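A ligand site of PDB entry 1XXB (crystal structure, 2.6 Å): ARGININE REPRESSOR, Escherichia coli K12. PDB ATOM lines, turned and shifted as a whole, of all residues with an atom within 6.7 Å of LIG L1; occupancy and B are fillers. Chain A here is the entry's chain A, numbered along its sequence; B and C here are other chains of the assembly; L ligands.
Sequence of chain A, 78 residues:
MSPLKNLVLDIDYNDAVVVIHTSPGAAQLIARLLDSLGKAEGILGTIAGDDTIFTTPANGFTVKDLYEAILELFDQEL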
ATOM      1  N   ALA A  27      28.289 -12.958 -19.502  1.00  0.00           N
ATOM      2  CA  ALA A  27      27.281 -14.026 -19.599  1.00  0.00           C
ATOM      3  C   ALA A  27      25.842 -13.528 -19.612  1.00  0.00           C
ATOM      4  O   ALA A  27      25.003 -14.098 -20.301  1.00  0.00           O
ATOM      5  CB  ALA A  27      27.458 -15.025 -18.458  1.00  0.00           C
ATOM      6  N   GLN A  28      25.572 -12.510 -18.806  1.00  0.00           N
ATOM      7  CA  GLN A  28      24.241 -11.907 -18.672  1.00  0.00           C
ATOM      8  C   GLN A  28      23.915 -10.998 -19.858  1.00  0.00           C
ATOM      9  O   GLN A  28      22.746 -10.696 -20.103  1.00  0.00           O
ATOM     10  CB  GLN A  28      24.147 -11.086 -17.376  1.00  0.00           C
ATOM     11  CG  GLN A  28      23.877 -11.888 -16.115  1.00  0.00           C
ATOM     12  CD  GLN A  28      22.427 -12.376 -15.994  1.00  0.00           C
ATOM     13  OE1 GLN A  28      21.554 -11.961 -16.763  1.00  0.00           O
ATOM     14  NE2 GLN A  28      22.182 -13.267 -15.039  1.00  0.00           N
ATOM     15  N   LEU A  29      24.952 -10.533 -20.541  1.00  0.00           N
ATOM     16  CA  LEU A  29      24.790  -9.654 -21.697  1.00  0.00           C
ATOM     17  C   LEU A  29      24.525 -10.467 -22.973  1.00  0.00           C
ATOM     18  O   LEU A  29      23.629 -10.123 -23.762  1.00  0.00           O
ATOM     19  CB  LEU A  29      26.028  -8.792 -21.884  1.00  0.00           C
ATOM     20  CG  LEU A  29      25.795  -7.410 -22.493  1.00  0.00           C
ATOM     21  CD1 LEU A  29      26.969  -7.147 -23.381  1.00  0.00           C
ATOM     22  CD2 LEU A  29      24.475  -7.296 -23.304  1.00  0.00           C
ATOM     23  N   ILE A  30      25.336 -11.494 -23.193  1.00  0.00           N
ATOM     24  CA  ILE A  30      25.186 -12.385 -24.339  1.00  0.00           C
ATOM     25  C   ILE A  30      23.964 -13.266 -24.153  1.00  0.00           C
ATOM     26  O   ILE A  30      23.230 -13.536 -25.107  1.00  0.00           O
ATOM     27  CB  ILE A  30      26.455 -13.229 -24.540  1.00  0.00           C
ATOM     28  CG1 ILE A  30      27.559 -12.336 -25.076  1.00  0.00           C
ATOM     29  CG2 ILE A  30      26.192 -14.393 -25.479  1.00  0.00           C
ATOM     30  CD1 ILE A  30      27.130 -11.529 -26.286  1.00  0.00           C
ATOM     31  N   ALA A  31      23.726 -13.726 -22.920  1.00  0.00           N
ATOM     32  CA  ALA A  31      22.540 -14.524 -22.616  1.00  0.00           C
ATOM     33  C   ALA A  31      21.325 -13.664 -23.000  1.00  0.00           C
ATOM     34  O   ALA A  31      20.278 -14.179 -23.421  1.00  0.00           O
ATOM     35  CB  ALA A  31      22.480 -14.845 -21.146  1.00  0.00           C
ATOM     36  N   ARG A  32      21.495 -12.355 -22.852  1.00  0.00           N
ATOM     37  CA  ARG A  32      20.476 -11.358 -23.154  1.00  0.00           C
ATOM     38  C   ARG A  32      20.193 -11.320 -24.643  1.00  0.00           C
ATOM     39  O   ARG A  32      19.082 -11.048 -25.068  1.00  0.00           O
ATOM     40  CB  ARG A  32      20.970 -10.010 -22.659  1.00  0.00           C
ATOM     41  CG  ARG A  32      20.037  -8.889 -22.913  1.00  0.00           C
ATOM     42  CD  ARG A  32      20.506  -7.681 -22.125  1.00  0.00           C
ATOM     43  NE  ARG A  32      19.942  -6.460 -22.669  1.00  0.00           N
ATOM     44  CZ  ARG A  32      18.642  -6.248 -22.855  1.00  0.00           C
ATOM     45  NH1 ARG A  32      17.744  -7.184 -22.527  1.00  0.00           N
ATOM     46  NH2 ARG A  32      18.232  -5.112 -23.400  1.00  0.00           N
ATOM     47  N   LEU A  33      21.221 -11.591 -25.444  1.00  0.00           N
ATOM     48  CA  LEU A  33      21.089 -11.643 -26.889  1.00  0.00           C
ATOM     49  C   LEU A  33      20.096 -12.755 -27.174  1.00  0.00           C
ATOM     50  O   LEU A  33      19.127 -12.545 -27.873  1.00  0.00           O
ATOM     51  CB  LEU A  33      22.424 -11.983 -27.545  1.00  0.00           C
ATOM     52  CG  LEU A  33      23.140 -10.852 -28.293  1.00  0.00           C
ATOM     53  CD1 LEU A  33      24.505 -11.306 -28.777  1.00  0.00           C
ATOM     54  CD2 LEU A  33      22.283 -10.407 -29.480  1.00  0.00           C
ATOM     55  N   ASP A  35      17.771 -14.021 -25.429  1.00  0.00           N
ATOM     56  CA  ASP A  35      16.409 -13.725 -25.044  1.00  0.00           C
ATOM     57  C   ASP A  35      15.677 -12.935 -26.131  1.00  0.00           C
ATOM     58  O   ASP A  35      14.510 -12.574 -25.966  1.00  0.00           O
ATOM     59  CB  ASP A  35      16.410 -12.982 -23.699  1.00  0.00           C
ATOM     60  CG  ASP A  35      16.930 -13.833 -22.542  1.00  0.00           C
ATOM     61  OD1 ASP A  35      17.973 -14.484 -22.680  1.00  0.00           O
ATOM     62  OD2 ASP A  35      16.275 -13.857 -21.490  1.00  0.00           O
ATOM     63  N   GLY A  45      14.525 -21.433 -22.706  1.00  0.00           N
ATOM     64  CA  GLY A  45      14.949 -20.555 -21.633  1.00  0.00           C
ATOM     65  C   GLY A  45      16.458 -20.396 -21.595  1.00  0.00           C
ATOM     66  O   GLY A  45      17.172 -21.213 -22.179  1.00  0.00           O
ATOM     67  N   THR A  46      16.946 -19.414 -20.852  1.00  0.00           N
ATOM     68  CA  THR A  46      18.376 -19.183 -20.771  1.00  0.00           C
ATOM     69  C   THR A  46      18.728 -18.594 -19.423  1.00  0.00           C
ATOM     70  O   THR A  46      18.009 -17.726 -18.902  1.00  0.00           O
ATOM     71  CB  THR A  46      18.791 -18.209 -21.884  1.00  0.00           C
ATOM     72  OG1 THR A  46      18.481 -18.771 -23.165  1.00  0.00           O
ATOM     73  CG2 THR A  46      20.287 -17.903 -21.813  1.00  0.00           C
ATOM     74  N   ILE A  47      19.793 -19.109 -18.824  1.00  0.00           N
ATOM     75  CA  ILE A  47      20.314 -18.668 -17.536  1.00  0.00           C
ATOM     76  C   ILE A  47      21.803 -18.385 -17.694  1.00  0.00           C
ATOM     77  O   ILE A  47      22.536 -19.204 -18.231  1.00  0.00           O
ATOM     78  CB  ILE A  47      20.193 -19.753 -16.451  1.00  0.00           C
ATOM     79  CG1 ILE A  47      18.735 -20.043 -16.162  1.00  0.00           C
ATOM     80  CG2 ILE A  47      20.854 -19.319 -15.150  1.00  0.00           C
ATOM     81  CD1 ILE A  47      18.569 -20.915 -14.966  1.00  0.00           C
ATOM     82  N   ALA A  48      22.233 -17.240 -17.188  1.00  0.00           N
ATOM     83  CA  ALA A  48      23.624 -16.871 -17.256  1.00  0.00           C
ATOM     84  C   ALA A  48      24.087 -16.698 -15.818  1.00  0.00           C
ATOM     85  O   ALA A  48      23.292 -16.391 -14.933  1.00  0.00           O
ATOM     86  CB  ALA A  48      23.772 -15.569 -18.015  1.00  0.00           C
ATOM     87  N   GLY A  49      25.353 -16.988 -15.570  1.00  0.00           N
ATOM     88  CA  GLY A  49      25.919 -16.820 -14.238  1.00  0.00           C
ATOM     89  C   GLY A  49      26.828 -15.603 -14.351  1.00  0.00           C
ATOM     90  O   GLY A  49      26.351 -14.480 -14.485  1.00  0.00           O
ATOM     91  N   ILE A  53      26.530 -19.757 -19.744  1.00  0.00           N
ATOM     92  CA  ILE A  53      25.130 -19.654 -20.092  1.00  0.00           C
ATOM     93  C   ILE A  53      24.585 -21.023 -20.445  1.00  0.00           C
ATOM     94  O   ILE A  53      25.161 -21.717 -21.273  1.00  0.00           O
ATOM     95  CB  ILE A  53      25.015 -18.750 -21.308  1.00  0.00           C
ATOM     96  CG1 ILE A  53      25.649 -17.384 -21.008  1.00  0.00           C
ATOM     97  CG2 ILE A  53      23.576 -18.617 -21.733  1.00  0.00           C
ATOM     98  CD1 ILE A  53      26.432 -16.814 -22.158  1.00  0.00           C
ATOM     99  N   HIS B  21       9.724 -18.368 -16.329  1.00  0.00           N
ATOM    100  CA  HIS B  21      10.028 -17.012 -16.796  1.00  0.00           C
ATOM    101  C   HIS B  21       9.306 -16.007 -15.910  1.00  0.00           C
ATOM    102  O   HIS B  21       8.088 -16.087 -15.745  1.00  0.00           O
ATOM    103  CB  HIS B  21       9.567 -16.779 -18.242  1.00  0.00           C
ATOM    104  CG  HIS B  21      10.509 -17.326 -19.279  1.00  0.00           C
ATOM    105  ND1 HIS B  21      10.296 -18.541 -19.869  1.00  0.00           N
ATOM    106  CD2 HIS B  21      11.682 -16.804 -19.716  1.00  0.00           C
ATOM    107  CE1 HIS B  21      11.337 -18.744 -20.648  1.00  0.00           C
ATOM    108  NE2 HIS B  21      12.209 -17.723 -20.592  1.00  0.00           N
ATOM    109  N   PRO B  24      11.546  -9.127 -14.726  1.00  0.00           N
ATOM    110  CA  PRO B  24      12.984  -8.955 -14.494  1.00  0.00           C
ATOM    111  C   PRO B  24      13.309  -8.664 -13.019  1.00  0.00           C
ATOM    112  O   PRO B  24      12.645  -7.868 -12.350  1.00  0.00           O
ATOM    113  CB  PRO B  24      13.313  -7.769 -15.377  1.00  0.00           C
ATOM    114  CG  PRO B  24      12.307  -7.901 -16.510  1.00  0.00           C
ATOM    115  CD  PRO B  24      11.052  -8.211 -15.743  1.00  0.00           C
ATOM    116  N   GLY B  25      14.337  -9.354 -12.517  1.00  0.00           N
ATOM    117  CA  GLY B  25      14.749  -9.168 -11.143  1.00  0.00           C
ATOM    118  C   GLY B  25      14.021 -10.052 -10.145  1.00  0.00           C
ATOM    119  O   GLY B  25      14.491 -10.228  -9.004  1.00  0.00           O
ATOM    120  N   ALA B  27      13.657 -13.305 -10.391  1.00  0.00           N
ATOM    121  CA  ALA B  27      14.112 -14.692 -10.462  1.00  0.00           C
ATOM    122  C   ALA B  27      14.432 -15.294  -9.114  1.00  0.00           C
ATOM    123  O   ALA B  27      13.718 -16.193  -8.658  1.00  0.00           O
ATOM    124  CB  ALA B  27      15.296 -14.825 -11.367  1.00  0.00           C
ATOM    125  N   ALA B  48      18.347 -19.740 -10.570  1.00  0.00           N
ATOM    126  CA  ALA B  48      17.690 -18.521 -11.015  1.00  0.00           C
ATOM    127  C   ALA B  48      18.662 -17.483 -11.566  1.00  0.00           C
ATOM    128  O   ALA B  48      19.801 -17.357 -11.084  1.00  0.00           O
ATOM    129  CB  ALA B  48      16.879 -17.930  -9.869  1.00  0.00           C
ATOM    130  N   GLY B  49      18.240 -16.783 -12.603  1.00  0.00           N
ATOM    131  CA  GLY B  49      19.067 -15.752 -13.191  1.00  0.00           C
ATOM    132  C   GLY B  49      18.458 -14.420 -12.815  1.00  0.00           C
ATOM    133  O   GLY B  49      18.339 -14.121 -11.620  1.00  0.00           O
ATOM    134  N   ASP B  50      18.107 -13.614 -13.824  1.00  0.00           N
ATOM    135  CA  ASP B  50      17.465 -12.301 -13.630  1.00  0.00           C
ATOM    136  C   ASP B  50      15.958 -12.479 -13.844  1.00  0.00           C
ATOM    137  O   ASP B  50      15.141 -11.974 -13.055  1.00  0.00           O
ATOM    138  CB  ASP B  50      18.014 -11.274 -14.622  1.00  0.00           C
ATOM    139  CG  ASP B  50      17.389  -9.881 -14.472  1.00  0.00           C
ATOM    140  OD1 ASP B  50      17.795  -9.184 -13.505  1.00  0.00           O
ATOM    141  OD2 ASP B  50      16.525  -9.467 -15.302  1.00  0.00           O
ATOM    142  N   ASP B  51      15.605 -13.240 -14.885  1.00  0.00           N
ATOM    143  CA  ASP B  51      14.219 -13.496 -15.265  1.00  0.00           C
ATOM    144  C   ASP B  51      13.883 -14.921 -15.717  1.00  0.00           C
ATOM    145  O   ASP B  51      12.798 -15.154 -16.274  1.00  0.00           O
ATOM    146  CB  ASP B  51      13.815 -12.514 -16.351  1.00  0.00           C
ATOM    147  CG  ASP B  51      14.878 -12.353 -17.396  1.00  0.00           C
ATOM    148  OD1 ASP B  51      15.373 -13.387 -17.891  1.00  0.00           O
ATOM    149  OD2 ASP B  51      15.254 -11.189 -17.663  1.00  0.00           O
ATOM    150  N   THR B  52      14.802 -15.855 -15.488  1.00  0.00           N
ATOM    151  CA  THR B  52      14.618 -17.265 -15.825  1.00  0.00           C
ATOM    152  C   THR B  52      15.004 -18.119 -14.618  1.00  0.00           C
ATOM    153  O   THR B  52      15.816 -17.711 -13.767  1.00  0.00           O
ATOM    154  CB  THR B  52      15.501 -17.685 -16.983  1.00  0.00           C
ATOM    155  OG1 THR B  52      15.526 -16.642 -17.946  1.00  0.00           O
ATOM    156  CG2 THR B  52      14.972 -18.949 -17.622  1.00  0.00           C
ATOM    157  N   ILE B  53      14.438 -19.311 -14.543  1.00  0.00           N
ATOM    158  CA  ILE B  53      14.707 -20.220 -13.444  1.00  0.00           C
ATOM    159  C   ILE B  53      14.709 -21.612 -14.054  1.00  0.00           C
ATOM    160  O   ILE B  53      13.747 -21.982 -14.726  1.00  0.00           O
ATOM    161  CB  ILE B  53      13.557 -20.156 -12.414  1.00  0.00           C
ATOM    162  CG1 ILE B  53      13.326 -18.704 -11.954  1.00  0.00           C
ATOM    163  CG2 ILE B  53      13.792 -21.117 -11.267  1.00  0.00           C
ATOM    164  CD1 ILE B  53      12.179 -18.592 -10.969  1.00  0.00           C
ATOM    165  N   PRO C  24      21.042  -3.395 -19.848  1.00  0.00           N
ATOM    166  CA  PRO C  24      20.807  -4.595 -19.045  1.00  0.00           C
ATOM    167  C   PRO C  24      21.913  -5.639 -19.089  1.00  0.00           C
ATOM    168  O   PRO C  24      22.402  -5.981 -20.159  1.00  0.00           O
ATOM    169  CB  PRO C  24      19.512  -5.149 -19.646  1.00  0.00           C
ATOM    170  CG  PRO C  24      18.795  -3.916 -20.094  1.00  0.00           C
ATOM    171  CD  PRO C  24      19.903  -3.132 -20.749  1.00  0.00           C
ATOM    172  N   GLY C  25      22.318  -6.135 -17.933  1.00  0.00           N
ATOM    173  CA  GLY C  25      23.359  -7.157 -17.873  1.00  0.00           C
ATOM    174  C   GLY C  25      24.778  -6.660 -18.068  1.00  0.00           C
ATOM    175  O   GLY C  25      25.738  -7.372 -17.755  1.00  0.00           O
ATOM    176  N   ALA C  26      24.907  -5.427 -18.554  1.00  0.00           N
ATOM    177  CA  ALA C  26      26.214  -4.808 -18.812  1.00  0.00           C
ATOM    178  C   ALA C  26      26.951  -4.367 -17.567  1.00  0.00           C
ATOM    179  O   ALA C  26      28.182  -4.321 -17.554  1.00  0.00           O
ATOM    180  CB  ALA C  26      26.062  -3.605 -19.753  1.00  0.00           C
ATOM    181  N   ASP C  50      22.711  -4.885 -11.833  1.00  0.00           N
ATOM    182  CA  ASP C  50      22.345  -5.412 -13.147  1.00  0.00           C
ATOM    183  C   ASP C  50      22.543  -4.396 -14.251  1.00  0.00           C
ATOM    184  O   ASP C  50      22.805  -4.770 -15.384  1.00  0.00           O
ATOM    185  CB  ASP C  50      20.899  -5.918 -13.168  1.00  0.00           C
ATOM    186  CG  ASP C  50      20.540  -6.578 -14.497  1.00  0.00           C
ATOM    187  OD1 ASP C  50      21.435  -7.113 -15.193  1.00  0.00           O
ATOM    188  OD2 ASP C  50      19.345  -6.576 -14.841  1.00  0.00           O
ATOM    189  N   ASP C  51      22.421  -3.107 -13.930  1.00  0.00           N
ATOM    190  CA  ASP C  51      22.597  -2.054 -14.925  1.00  0.00           C
ATOM    191  C   ASP C  51      23.193  -0.763 -14.377  1.00  0.00           C
ATOM    192  O   ASP C  51      23.266   0.235 -15.079  1.00  0.00           O
ATOM    193  CB  ASP C  51      21.270  -1.770 -15.643  1.00  0.00           C
ATOM    194  CG  ASP C  51      20.110  -1.482 -14.686  1.00  0.00           C
ATOM    195  OD1 ASP C  51      20.332  -0.846 -13.640  1.00  0.00           O
ATOM    196  OD2 ASP C  51      18.963  -1.866 -14.994  1.00  0.00           O
HETATM  197  N1  LIG L   1      17.532 -14.777 -18.722  1.00  0.00           N
HETATM  198  C1  LIG L   1      19.006 -14.796 -18.669  1.00  0.00           C
HETATM  199  C2  LIG L   1      19.430 -14.963 -17.245  1.00  0.00           C
HETATM  200  O1  LIG L   1      20.644 -15.058 -17.001  1.00  0.00           O
HETATM  201  C3  LIG L   1      19.569 -13.488 -19.210  1.00  0.00           C
HETATM  202  C4  LIG L   1      19.062 -12.243 -18.519  1.00  0.00           C
HETATM  203  C5  LIG L   1      19.725 -11.009 -19.080  1.00  0.00           C
HETATM  204  N2  LIG L   1      19.080  -9.801 -18.596  1.00  0.00           N
HETATM  205  C6  LIG L   1      19.507  -9.089 -17.567  1.00  0.00           C
HETATM  206  N3  LIG L   1      20.605  -9.445 -16.920  1.00  0.00           N
HETATM  207  N4  LIG L   1      18.817  -8.032 -17.158  1.00  0.00           N
HETATM  208  O2  LIG L   1      18.524 -14.981 -16.381  1.00  0.00           O
HETATM  209  N1  LG2 L   2      19.497  -0.709 -10.656  1.00  0.00           N
HETATM  210  C1  LG2 L   2      19.553  -1.884  -9.742  1.00  0.00           C
HETATM  211  C2  LG2 L   2      20.736  -2.772 -10.108  1.00  0.00           C
HETATM  212  O1  LG2 L   2      20.875  -3.845  -9.478  1.00  0.00           O
HETATM  213  C3  LG2 L   2      18.274  -2.683  -9.871  1.00  0.00           C
HETATM  214  C4  LG2 L   2      18.086  -3.328 -11.206  1.00  0.00           C
HETATM  215  C5  LG2 L   2      16.813  -4.113 -11.142  1.00  0.00           C
HETATM  216  N2  LG2 L   2      16.469  -4.763 -12.396  1.00  0.00           N
HETATM  217  C6  LG2 L   2      16.963  -5.919 -12.809  1.00  0.00           C
HETATM  218  N3  LG2 L   2      17.823  -6.573 -12.062  1.00  0.00           N
HETATM  219  N4  LG2 L   2      16.539  -6.460 -13.942  1.00  0.00           N
HETATM  220  O2  LG2 L   2      21.492  -2.420 -11.019  1.00  0.00           O
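A nitrogen (N4) of LIG L1 is in salt-bridge range of the side-chain carboxylate of Asp 50 of chain C (2.8 Å). The side-chain carboxylate (OD2) of Asp 50 of chain B is in salt-bridge range of a nitrogen (N4) of LIG L1 (3.3 Å). The backbone carbonyl oxygen of Thr 46 is in hydrogen-bond range of a nitrogen (N1) of LIG L1. A nitrogen (N1) of LIG L1 is in salt-bridge range of the side-chain carboxylate (OD1) of Asp 51 of chain B (2.7 Å). The side-chain carboxylate (OD1) of Asp 50 of chain B lies within salt-bridge range of a nitrogen (N3) of LG2 L2, 3.0 Å away. The backbone NH of Asp 50 of chain C sits at hydrogen-bond distance from an oxygen (O2) of LG2 L2 (2.9 Å). The side-chain carboxylate (OD2) of Asp 50 of chain C is in salt-bridge range of a nitrogen (N4) of LG2 L2 (2.9 Å). An oxygen (O1) of LIG L1 sits at hydrogen-bond distance from the backbone NH (N) of Ala 48 of chain A (2.7 Å). OE1 of Gln 28 lies within hydrogen-bond range of N3 of LIG L1. An oxygen (O2) of LIG L1 is in hydrogen-bond range of the backbone NH (N) of Asp 50 of chain B (2.9 Å). The side-chain hydroxyl (OG1) of Thr 52 of chain B lies within hydrogen-bond range of a nitrogen (N1) of LIG L1, at 2.8 Å. OD2 of Asp 35 lies within salt-bridge range of N1 of LIG L1.
The backbone carbonyl oxygen of Thr 46 sits at hydrogen-bond distance from the side-chain hydroxyl of Thr 52 of chain B, at 2.9 Å. The backbone carbonyl oxygen (O) of Ala 31 lies close to the side-chain carboxylate (OD1) of Asp 35 (2.4 Å). O of Ala 48 of chain A sits at hydrogen-bond distance from NE2 of Gln 28. The backbone NH (N) of Gly 25 of chain C sits at hydrogen-bond distance from the backbone carbonyl oxygen (O) of Asp 50 of chain C (2.9 Å). O of Asp 50 of chain B sits close to N of Ala 27 of chain B. The side-chain carboxylate of Asp 51 of chain B sits at hydrogen-bond distance from the side-chain hydroxyl of Thr 52 of chain B, 3.3 Å away.
Ala 31 touches LIG L1 (CB to C3, 3.8 Å). CB of Arg 32 touches C5 of LIG L1, at 3.9 Å. Ile 47 touches LIG L1 (C to O1, 3.6 Å). CA of Gly 49 of chain B touches O2 of LIG L1, 3.3 Å away. Pro 24 of chain C touches LIG L1. CA of Gly 25 of chain C touches N3 of LIG L1, at 3.7 Å. Hydrophobic or aromatic side chains that line LIG L1: Ala 31, Ala 48 of chain A and Pro 24 of chain C. Of the 29 residues printed, 14 come within 4 Å of LIG L1. The nearest printed residue that does not touch LIG L1 is Gly 49 of chain A (5.3 Å).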
